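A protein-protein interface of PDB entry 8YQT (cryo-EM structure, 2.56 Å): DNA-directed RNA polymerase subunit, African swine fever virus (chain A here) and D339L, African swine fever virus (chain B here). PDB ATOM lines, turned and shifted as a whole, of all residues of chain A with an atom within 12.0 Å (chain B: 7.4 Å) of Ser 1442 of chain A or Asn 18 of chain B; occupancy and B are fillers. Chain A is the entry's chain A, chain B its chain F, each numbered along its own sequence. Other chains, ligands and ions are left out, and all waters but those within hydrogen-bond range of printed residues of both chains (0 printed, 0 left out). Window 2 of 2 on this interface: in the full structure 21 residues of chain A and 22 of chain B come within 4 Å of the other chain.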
ATOM      1  N   GLN A 355     -21.586 -24.618  23.109  1.00  0.00           N
ATOM      2  CA  GLN A 355     -21.917 -24.540  21.694  1.00  0.00           C
ATOM      3  C   GLN A 355     -21.412 -25.810  21.024  1.00  0.00           C
ATOM      4  O   GLN A 355     -20.916 -26.728  21.681  1.00  0.00           O
ATOM      5  CB  GLN A 355     -21.326 -23.275  21.057  1.00  0.00           C
ATOM      6  CG  GLN A 355     -22.107 -22.008  21.337  1.00  0.00           C
ATOM      7  CD  GLN A 355     -23.534 -22.078  20.837  1.00  0.00           C
ATOM      8  OE1 GLN A 355     -24.480 -21.886  21.597  1.00  0.00           O
ATOM      9  NE2 GLN A 355     -23.697 -22.362  19.551  1.00  0.00           N
ATOM     10  N   ILE A1430     -22.016  -1.547  14.251  1.00  0.00           N
ATOM     11  CA  ILE A1430     -23.297  -1.872  13.646  1.00  0.00           C
ATOM     12  C   ILE A1430     -23.140  -3.159  12.852  1.00  0.00           C
ATOM     13  O   ILE A1430     -22.047  -3.521  12.414  1.00  0.00           O
ATOM     14  CB  ILE A1430     -23.838  -0.736  12.753  1.00  0.00           C
ATOM     15  CG1 ILE A1430     -22.960  -0.551  11.521  1.00  0.00           C
ATOM     16  CG2 ILE A1430     -23.928   0.553  13.531  1.00  0.00           C
ATOM     17  CD1 ILE A1430     -23.468   0.496  10.569  1.00  0.00           C
ATOM     18  N   MET A1431     -24.253  -3.860  12.684  1.00  0.00           N
ATOM     19  CA  MET A1431     -24.250  -5.113  11.950  1.00  0.00           C
ATOM     20  C   MET A1431     -24.092  -4.833  10.462  1.00  0.00           C
ATOM     21  O   MET A1431     -24.662  -3.874   9.935  1.00  0.00           O
ATOM     22  CB  MET A1431     -25.546  -5.876  12.206  1.00  0.00           C
ATOM     23  CG  MET A1431     -25.634  -6.547  13.569  1.00  0.00           C
ATOM     24  SD  MET A1431     -24.161  -7.431  14.090  1.00  0.00           S
ATOM     25  CE  MET A1431     -24.404  -9.007  13.294  1.00  0.00           C
ATOM     26  N   ASP A1432     -23.312  -5.670   9.784  1.00  0.00           N
ATOM     27  CA  ASP A1432     -23.092  -5.525   8.346  1.00  0.00           C
ATOM     28  C   ASP A1432     -24.179  -6.308   7.619  1.00  0.00           C
ATOM     29  O   ASP A1432     -24.026  -7.500   7.350  1.00  0.00           O
ATOM     30  CB  ASP A1432     -21.699  -6.004   7.959  1.00  0.00           C
ATOM     31  CG  ASP A1432     -21.269  -5.497   6.600  1.00  0.00           C
ATOM     32  OD1 ASP A1432     -22.092  -4.858   5.913  1.00  0.00           O
ATOM     33  OD2 ASP A1432     -20.105  -5.732   6.218  1.00  0.00           O
ATOM     34  N   GLU A1433     -25.282  -5.630   7.297  1.00  0.00           N
ATOM     35  CA  GLU A1433     -26.419  -6.305   6.682  1.00  0.00           C
ATOM     36  C   GLU A1433     -26.095  -6.779   5.270  1.00  0.00           C
ATOM     37  O   GLU A1433     -26.417  -7.915   4.905  1.00  0.00           O
ATOM     38  CB  GLU A1433     -27.628  -5.376   6.662  1.00  0.00           C
ATOM     39  CG  GLU A1433     -27.954  -4.758   8.002  1.00  0.00           C
ATOM     40  CD  GLU A1433     -29.059  -3.733   7.904  1.00  0.00           C
ATOM     41  OE1 GLU A1433     -29.740  -3.697   6.859  1.00  0.00           O
ATOM     42  OE2 GLU A1433     -29.244  -2.961   8.868  1.00  0.00           O
ATOM     43  N   LYS A1434     -25.461  -5.927   4.463  1.00  0.00           N
ATOM     44  CA  LYS A1434     -25.140  -6.292   3.089  1.00  0.00           C
ATOM     45  C   LYS A1434     -24.207  -7.492   3.011  1.00  0.00           C
ATOM     46  O   LYS A1434     -24.189  -8.185   1.990  1.00  0.00           O
ATOM     47  CB  LYS A1434     -24.524  -5.092   2.366  1.00  0.00           C
ATOM     48  CG  LYS A1434     -24.365  -5.254   0.864  1.00  0.00           C
ATOM     49  CD  LYS A1434     -22.916  -5.517   0.487  1.00  0.00           C
ATOM     50  CE  LYS A1434     -22.677  -5.309  -0.999  1.00  0.00           C
ATOM     51  NZ  LYS A1434     -23.408  -6.296  -1.838  1.00  0.00           N
ATOM     52  N   TYR A1435     -23.443  -7.760   4.067  1.00  0.00           N
ATOM     53  CA  TYR A1435     -22.555  -8.912   4.096  1.00  0.00           C
ATOM     54  C   TYR A1435     -23.231 -10.157   4.648  1.00  0.00           C
ATOM     55  O   TYR A1435     -22.965 -11.262   4.164  1.00  0.00           O
ATOM     56  CB  TYR A1435     -21.313  -8.588   4.929  1.00  0.00           C
ATOM     57  CG  TYR A1435     -20.209  -9.613   4.847  1.00  0.00           C
ATOM     58  CD1 TYR A1435     -19.447  -9.749   3.699  1.00  0.00           C
ATOM     59  CD2 TYR A1435     -19.913 -10.429   5.927  1.00  0.00           C
ATOM     60  CE1 TYR A1435     -18.435 -10.676   3.624  1.00  0.00           C
ATOM     61  CE2 TYR A1435     -18.902 -11.359   5.861  1.00  0.00           C
ATOM     62  CZ  TYR A1435     -18.165 -11.477   4.707  1.00  0.00           C
ATOM     63  OH  TYR A1435     -17.152 -12.403   4.631  1.00  0.00           O
ATOM     64  N   ILE A1436     -24.098 -10.007   5.648  1.00  0.00           N
ATOM     65  CA  ILE A1436     -24.742 -11.164   6.260  1.00  0.00           C
ATOM     66  C   ILE A1436     -25.753 -11.797   5.310  1.00  0.00           C
ATOM     67  O   ILE A1436     -25.855 -13.025   5.225  1.00  0.00           O
ATOM     68  CB  ILE A1436     -25.385 -10.758   7.596  1.00  0.00           C
ATOM     69  CG1 ILE A1436     -24.304 -10.401   8.615  1.00  0.00           C
ATOM     70  CG2 ILE A1436     -26.248 -11.870   8.134  1.00  0.00           C
ATOM     71  CD1 ILE A1436     -24.844  -9.788   9.875  1.00  0.00           C
ATOM     72  N   THR A1437     -26.511 -10.977   4.579  1.00  0.00           N
ATOM     73  CA  THR A1437     -27.493 -11.522   3.646  1.00  0.00           C
ATOM     74  C   THR A1437     -26.830 -12.307   2.524  1.00  0.00           C
ATOM     75  O   THR A1437     -27.391 -13.300   2.050  1.00  0.00           O
ATOM     76  CB  THR A1437     -28.349 -10.400   3.059  1.00  0.00           C
ATOM     77  OG1 THR A1437     -27.525  -9.529   2.275  1.00  0.00           O
ATOM     78  CG2 THR A1437     -29.008  -9.599   4.163  1.00  0.00           C
ATOM     79  N   GLU A1438     -25.645 -11.883   2.087  1.00  0.00           N
ATOM     80  CA  GLU A1438     -24.946 -12.513   0.976  1.00  0.00           C
ATOM     81  C   GLU A1438     -24.048 -13.665   1.400  1.00  0.00           C
ATOM     82  O   GLU A1438     -23.503 -14.352   0.532  1.00  0.00           O
ATOM     83  CB  GLU A1438     -24.105 -11.474   0.231  1.00  0.00           C
ATOM     84  CG  GLU A1438     -24.914 -10.343  -0.367  1.00  0.00           C
ATOM     85  CD  GLU A1438     -24.041  -9.276  -0.986  1.00  0.00           C
ATOM     86  OE1 GLU A1438     -22.803  -9.367  -0.847  1.00  0.00           O
ATOM     87  OE2 GLU A1438     -24.591  -8.344  -1.607  1.00  0.00           O
ATOM     88  N   ASN A1439     -23.873 -13.888   2.700  1.00  0.00           N
ATOM     89  CA  ASN A1439     -22.988 -14.945   3.179  1.00  0.00           C
ATOM     90  C   ASN A1439     -23.584 -15.825   4.265  1.00  0.00           C
ATOM     91  O   ASN A1439     -23.064 -16.923   4.485  1.00  0.00           O
ATOM     92  CB  ASN A1439     -21.671 -14.350   3.696  1.00  0.00           C
ATOM     93  CG  ASN A1439     -20.961 -13.500   2.656  1.00  0.00           C
ATOM     94  OD1 ASN A1439     -21.414 -12.412   2.310  1.00  0.00           O
ATOM     95  ND2 ASN A1439     -19.843 -14.000   2.151  1.00  0.00           N
ATOM     96  N   TYR A1440     -24.638 -15.404   4.958  1.00  0.00           N
ATOM     97  CA  TYR A1440     -25.239 -16.191   6.022  1.00  0.00           C
ATOM     98  C   TYR A1440     -26.674 -16.557   5.663  1.00  0.00           C
ATOM     99  O   TYR A1440     -27.275 -15.988   4.747  1.00  0.00           O
ATOM    100  CB  TYR A1440     -25.219 -15.437   7.357  1.00  0.00           C
ATOM    101  CG  TYR A1440     -23.840 -15.248   7.949  1.00  0.00           C
ATOM    102  CD1 TYR A1440     -22.775 -16.040   7.552  1.00  0.00           C
ATOM    103  CD2 TYR A1440     -23.608 -14.278   8.910  1.00  0.00           C
ATOM    104  CE1 TYR A1440     -21.519 -15.867   8.093  1.00  0.00           C
ATOM    105  CE2 TYR A1440     -22.356 -14.097   9.456  1.00  0.00           C
ATOM    106  CZ  TYR A1440     -21.315 -14.893   9.045  1.00  0.00           C
ATOM    107  OH  TYR A1440     -20.065 -14.714   9.590  1.00  0.00           O
ATOM    108  N   LYS A1441     -27.216 -17.522   6.402  1.00  0.00           N
ATOM    109  CA  LYS A1441     -28.587 -17.974   6.233  1.00  0.00           C
ATOM    110  C   LYS A1441     -29.273 -18.037   7.590  1.00  0.00           C
ATOM    111  O   LYS A1441     -28.623 -18.153   8.633  1.00  0.00           O
ATOM    112  CB  LYS A1441     -28.654 -19.348   5.551  1.00  0.00           C
ATOM    113  CG  LYS A1441     -28.019 -19.400   4.175  1.00  0.00           C
ATOM    114  CD  LYS A1441     -28.739 -18.486   3.197  1.00  0.00           C
ATOM    115  CE  LYS A1441     -28.248 -18.707   1.777  1.00  0.00           C
ATOM    116  NZ  LYS A1441     -26.821 -18.318   1.615  1.00  0.00           N
ATOM    117  N   SER A1442     -30.599 -17.959   7.565  1.00  0.00           N
ATOM    118  CA  SER A1442     -31.397 -18.025   8.785  1.00  0.00           C
ATOM    119  C   SER A1442     -31.294 -19.400   9.440  1.00  0.00           C
ATOM    120  O   SER A1442     -31.672 -19.577  10.598  1.00  0.00           O
ATOM    121  CB  SER A1442     -32.862 -17.697   8.487  1.00  0.00           C
ATOM    122  OG  SER A1442     -33.009 -16.359   8.046  1.00  0.00           O
ATOM    123  N   ILE B  13     -32.908  -6.690  19.811  1.00  0.00           N
ATOM    124  CA  ILE B  13     -32.616  -7.776  18.885  1.00  0.00           C
ATOM    125  C   ILE B  13     -31.654  -8.715  19.598  1.00  0.00           C
ATOM    126  O   ILE B  13     -30.472  -8.395  19.763  1.00  0.00           O
ATOM    127  CB  ILE B  13     -32.023  -7.268  17.569  1.00  0.00           C
ATOM    128  CG1 ILE B  13     -33.018  -6.347  16.863  1.00  0.00           C
ATOM    129  CG2 ILE B  13     -31.650  -8.427  16.685  1.00  0.00           C
ATOM    130  CD1 ILE B  13     -32.413  -5.521  15.772  1.00  0.00           C
ATOM    131  N   ASP B  14     -32.151  -9.874  20.020  1.00  0.00           N
ATOM    132  CA  ASP B  14     -31.336 -10.821  20.768  1.00  0.00           C
ATOM    133  C   ASP B  14     -30.343 -11.571  19.891  1.00  0.00           C
ATOM    134  O   ASP B  14     -29.297 -11.998  20.390  1.00  0.00           O
ATOM    135  CB  ASP B  14     -32.238 -11.813  21.497  1.00  0.00           C
ATOM    136  CG  ASP B  14     -33.369 -11.129  22.228  1.00  0.00           C
ATOM    137  OD1 ASP B  14     -33.192 -10.795  23.418  1.00  0.00           O
ATOM    138  OD2 ASP B  14     -34.434 -10.916  21.613  1.00  0.00           O
ATOM    139  N   ASP B  15     -30.642 -11.740  18.606  1.00  0.00           N
ATOM    140  CA  ASP B  15     -29.770 -12.466  17.686  1.00  0.00           C
ATOM    141  C   ASP B  15     -29.540 -11.601  16.457  1.00  0.00           C
ATOM    142  O   ASP B  15     -30.185 -11.789  15.419  1.00  0.00           O
ATOM    143  CB  ASP B  15     -30.372 -13.816  17.303  1.00  0.00           C
ATOM    144  CG  ASP B  15     -29.350 -14.769  16.730  1.00  0.00           C
ATOM    145  OD1 ASP B  15     -29.625 -15.984  16.706  1.00  0.00           O
ATOM    146  OD2 ASP B  15     -28.271 -14.307  16.304  1.00  0.00           O
ATOM    147  N   PRO B  16     -28.628 -10.630  16.543  1.00  0.00           N
ATOM    148  CA  PRO B  16     -28.430  -9.711  15.412  1.00  0.00           C
ATOM    149  C   PRO B  16     -28.006 -10.402  14.128  1.00  0.00           C
ATOM    150  O   PRO B  16     -28.427  -9.977  13.045  1.00  0.00           O
ATOM    151  CB  PRO B  16     -27.342  -8.757  15.925  1.00  0.00           C
ATOM    152  CG  PRO B  16     -27.399  -8.876  17.403  1.00  0.00           C
ATOM    153  CD  PRO B  16     -27.756 -10.293  17.679  1.00  0.00           C
ATOM    154  N   THR B  17     -27.195 -11.456  14.216  1.00  0.00           N
ATOM    155  CA  THR B  17     -26.734 -12.138  13.011  1.00  0.00           C
ATOM    156  C   THR B  17     -27.894 -12.781  12.261  1.00  0.00           C
ATOM    157  O   THR B  17     -28.022 -12.615  11.043  1.00  0.00           O
ATOM    158  CB  THR B  17     -25.689 -13.189  13.374  1.00  0.00           C
ATOM    159  OG1 THR B  17     -24.833 -12.678  14.402  1.00  0.00           O
ATOM    160  CG2 THR B  17     -24.852 -13.536  12.162  1.00  0.00           C
ATOM    161  N   ASN B  18     -28.747 -13.521  12.973  1.00  0.00           N
ATOM    162  CA  ASN B  18     -29.920 -14.113  12.341  1.00  0.00           C
ATOM    163  C   ASN B  18     -30.908 -13.043  11.901  1.00  0.00           C
ATOM    164  O   ASN B  18     -31.528 -13.160  10.838  1.00  0.00           O
ATOM    165  CB  ASN B  18     -30.586 -15.096  13.303  1.00  0.00           C
ATOM    166  CG  ASN B  18     -31.953 -15.538  12.827  1.00  0.00           C
ATOM    167  OD1 ASN B  18     -32.917 -15.548  13.593  1.00  0.00           O
ATOM    168  ND2 ASN B  18     -32.044 -15.915  11.557  1.00  0.00           N
ATOM    169  N   PHE B  19     -31.067 -11.991  12.708  1.00  0.00           N
ATOM    170  CA  PHE B  19     -32.022 -10.936  12.392  1.00  0.00           C
ATOM    171  C   PHE B  19     -31.661 -10.229  11.093  1.00  0.00           C
ATOM    172  O   PHE B  19     -32.543  -9.883  10.300  1.00  0.00           O
ATOM    173  CB  PHE B  19     -32.081  -9.933  13.542  1.00  0.00           C
ATOM    174  CG  PHE B  19     -33.123  -8.864  13.372  1.00  0.00           C
ATOM    175  CD1 PHE B  19     -34.407  -9.051  13.852  1.00  0.00           C
ATOM    176  CD2 PHE B  19     -32.817  -7.671  12.741  1.00  0.00           C
ATOM    177  CE1 PHE B  19     -35.364  -8.068  13.702  1.00  0.00           C
ATOM    178  CE2 PHE B  19     -33.770  -6.690  12.585  1.00  0.00           C
ATOM    179  CZ  PHE B  19     -35.044  -6.887  13.066  1.00  0.00           C
ATOM    180  N   CYS B  20     -30.372 -10.000  10.858  1.00  0.00           N
ATOM    181  CA  CYS B  20     -29.949  -9.201   9.717  1.00  0.00           C
ATOM    182  C   CYS B  20     -29.939  -9.974   8.405  1.00  0.00           C
ATOM    183  O   CYS B  20     -29.689  -9.369   7.358  1.00  0.00           O
ATOM    184  CB  CYS B  20     -28.566  -8.606   9.981  1.00  0.00           C
ATOM    185  SG  CYS B  20     -28.578  -7.309  11.228  1.00  0.00           S
ATOM    186  N   THR B  21     -30.195 -11.283   8.430  1.00  0.00           N
ATOM    187  CA  THR B  21     -30.307 -12.035   7.183  1.00  0.00           C
ATOM    188  C   THR B  21     -31.503 -11.578   6.357  1.00  0.00           C
ATOM    189  O   THR B  21     -31.408 -11.497   5.128  1.00  0.00           O
ATOM    190  CB  THR B  21     -30.407 -13.531   7.474  1.00  0.00           C
ATOM    191  OG1 THR B  21     -31.488 -13.771   8.383  1.00  0.00           O
ATOM    192  CG2 THR B  21     -29.118 -14.042   8.083  1.00  0.00           C
ATOM    193  N   ASN B  22     -32.635 -11.292   7.004  1.00  0.00           N
ATOM    194  CA  ASN B  22     -33.796 -10.729   6.310  1.00  0.00           C
ATOM    195  C   ASN B  22     -34.365  -9.631   7.212  1.00  0.00           C
ATOM    196  O   ASN B  22     -35.278  -9.871   8.007  1.00  0.00           O
ATOM    197  CB  ASN B  22     -34.831 -11.801   6.000  1.00  0.00           C
ATOM    198  CG  ASN B  22     -35.741 -11.417   4.855  1.00  0.00           C
ATOM    199  OD1 ASN B  22     -35.664 -10.306   4.331  1.00  0.00           O
ATOM    200  ND2 ASN B  22     -36.608 -12.337   4.458  1.00  0.00           N
ATOM    201  N   VAL B  23     -33.827  -8.419   7.051  1.00  0.00           N
ATOM    202  CA  VAL B  23     -34.121  -7.342   7.990  1.00  0.00           C
ATOM    203  C   VAL B  23     -35.577  -6.920   7.894  1.00  0.00           C
ATOM    204  O   VAL B  23     -36.253  -6.757   8.913  1.00  0.00           O
ATOM    205  CB  VAL B  23     -33.175  -6.150   7.761  1.00  0.00           C
ATOM    206  CG1 VAL B  23     -33.638  -4.949   8.564  1.00  0.00           C
ATOM    207  CG2 VAL B  23     -31.761  -6.517   8.146  1.00  0.00           C
ATOM    208  N   HIS B  26     -37.973  -9.766   9.229  1.00  0.00           N
ATOM    209  CA  HIS B  26     -37.886  -9.885  10.678  1.00  0.00           C
ATOM    210  C   HIS B  26     -38.458  -8.660  11.378  1.00  0.00           C
ATOM    211  O   HIS B  26     -39.118  -8.791  12.415  1.00  0.00           O
ATOM    212  CB  HIS B  26     -36.435 -10.117  11.095  1.00  0.00           C
ATOM    213  CG  HIS B  26     -35.902 -11.459  10.708  1.00  0.00           C
ATOM    214  ND1 HIS B  26     -35.374 -11.720   9.463  1.00  0.00           N
ATOM    215  CD2 HIS B  26     -35.812 -12.617  11.404  1.00  0.00           C
ATOM    216  CE1 HIS B  26     -34.982 -12.981   9.407  1.00  0.00           C
ATOM    217  NE2 HIS B  26     -35.237 -13.548  10.571  1.00  0.00           N
ATOM    218  N   LYS B  29     -42.227  -8.914  11.281  1.00  0.00           N
ATOM    219  CA  LYS B  29     -42.723  -9.933  12.201  1.00  0.00           C
ATOM    220  C   LYS B  29     -42.654  -9.460  13.650  1.00  0.00           C
ATOM    221  O   LYS B  29     -43.618  -9.625  14.409  1.00  0.00           O
ATOM    222  CB  LYS B  29     -41.942 -11.232  12.014  1.00  0.00           C
ATOM    223  CG  LYS B  29     -42.522 -12.414  12.768  1.00  0.00           C
ATOM    224  CD  LYS B  29     -41.871 -13.722  12.346  1.00  0.00           C
ATOM    225  CE  LYS B  29     -40.484 -13.872  12.944  1.00  0.00           C
ATOM    226  NZ  LYS B  29     -39.902 -15.210  12.652  1.00  0.00           N
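Of the printed residues of chain B, Glu 1433 of chain A touches Val 23 (3.7 Å).
Lys 1434 of chain A touches none of the printed residues of chain B.
Of the printed residues of chain B, Ile 1436 of chain A touches Thr 17 (3.5 Å), Cys 20 (3.9 Å) and Thr 21 (3.6 Å).
Of the printed residues of chain B, Thr 1437 of chain A touches Cys 20 and Thr 21.
Ile 13 of chain B touches none of the printed residues of chain A.
No residue of chain A comes within 4 Å of Asp 15 of chain B.
Of chain A, only Met 1431 (3.7 Å) comes within 4 Å of Pro 16 of chain B.
Cys 20 of chain B touches just these residues of chain A: Met 1431, Ile 1436 and Thr 1437.
Thr 21 of chain B touches just these residues of chain A: Ile 1436 (3.6 Å), Thr 1437 (3.2 Å) and Ser 1442 (3.0 Å).
No residue of chain A comes within 4 Å of Asn 22 of chain B.
Of the printed residues of chain A, Val 23 of chain B touches Glu 1433 (3.7 Å).
The nearest residue of chain B that does not touch Ser 1442 of chain A is His 26 of chain B (4.1 Å).
The nearest residue of chain A that does not touch Asn 18 of chain B is Lys 1441 of chain A (5.0 Å).
The nearest printed residue of chain B that does not touch Ile 1436 of chain A is Pro 16 of chain B (4.8 Å).
Of the 14 printed residues of chain A, 6 touch a printed residue of chain B.
Among the printed residues, no Asp or Glu carboxylate lies within 4 Å of a Lys or Arg side-chain nitrogen of the other chain.
The side-chain sulfur of Cys 20 of chain B lies within hydrogen-bond range of the backbone carbonyl oxygen of Pro 16 of chain B (3.2 Å).
OD2 of Asp 15 of chain B sits at hydrogen-bond distance from N of Asn 18 of chain B.
The backbone carbonyl oxygen of Glu 1433 of chain A sits close to the side-chain hydroxyl of Thr 1437 of chain A (3.3 Å).
The side-chain hydroxyl of Thr 21 of chain B is in hydrogen-bond range of the backbone carbonyl oxygen of Asn 18 of chain B, at 2.5 Å.
The side-chain hydroxyl (OG1) of Thr 21 of chain B lies within hydrogen-bond range of the side-chain hydroxyl (OG) of Ser 1442 of chain A (3.0 Å).
Among the printed residues, merely in contact across the chains: Thr 1437 of chain A with Thr 21 of chain B (3.2 Å), Thr 1437 of chain A with Cys 20 of chain B (3.3 Å), Ile 1436 of chain A with Thr 17 of chain B (3.5 Å), Met 1431 of chain A with Cys 20 of chain B (3.5 Å), Ser 1442 of chain A with Asn 18 of chain B (3.5 Å), Tyr 1440 of chain A with Thr 17 of chain B (3.6 Å), Ile 1436 of chain A with Thr 21 of chain B (3.6 Å), Met 1431 of chain A with Pro 16 of chain B (3.7 Å), Glu 1433 of chain A with Val 23 of chain B (3.7 Å), Met 1431 of chain A with Thr 17 of chain B (3.8 Å) and Ile 1436 of chain A with Cys 20 of chain B (3.9 Å).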
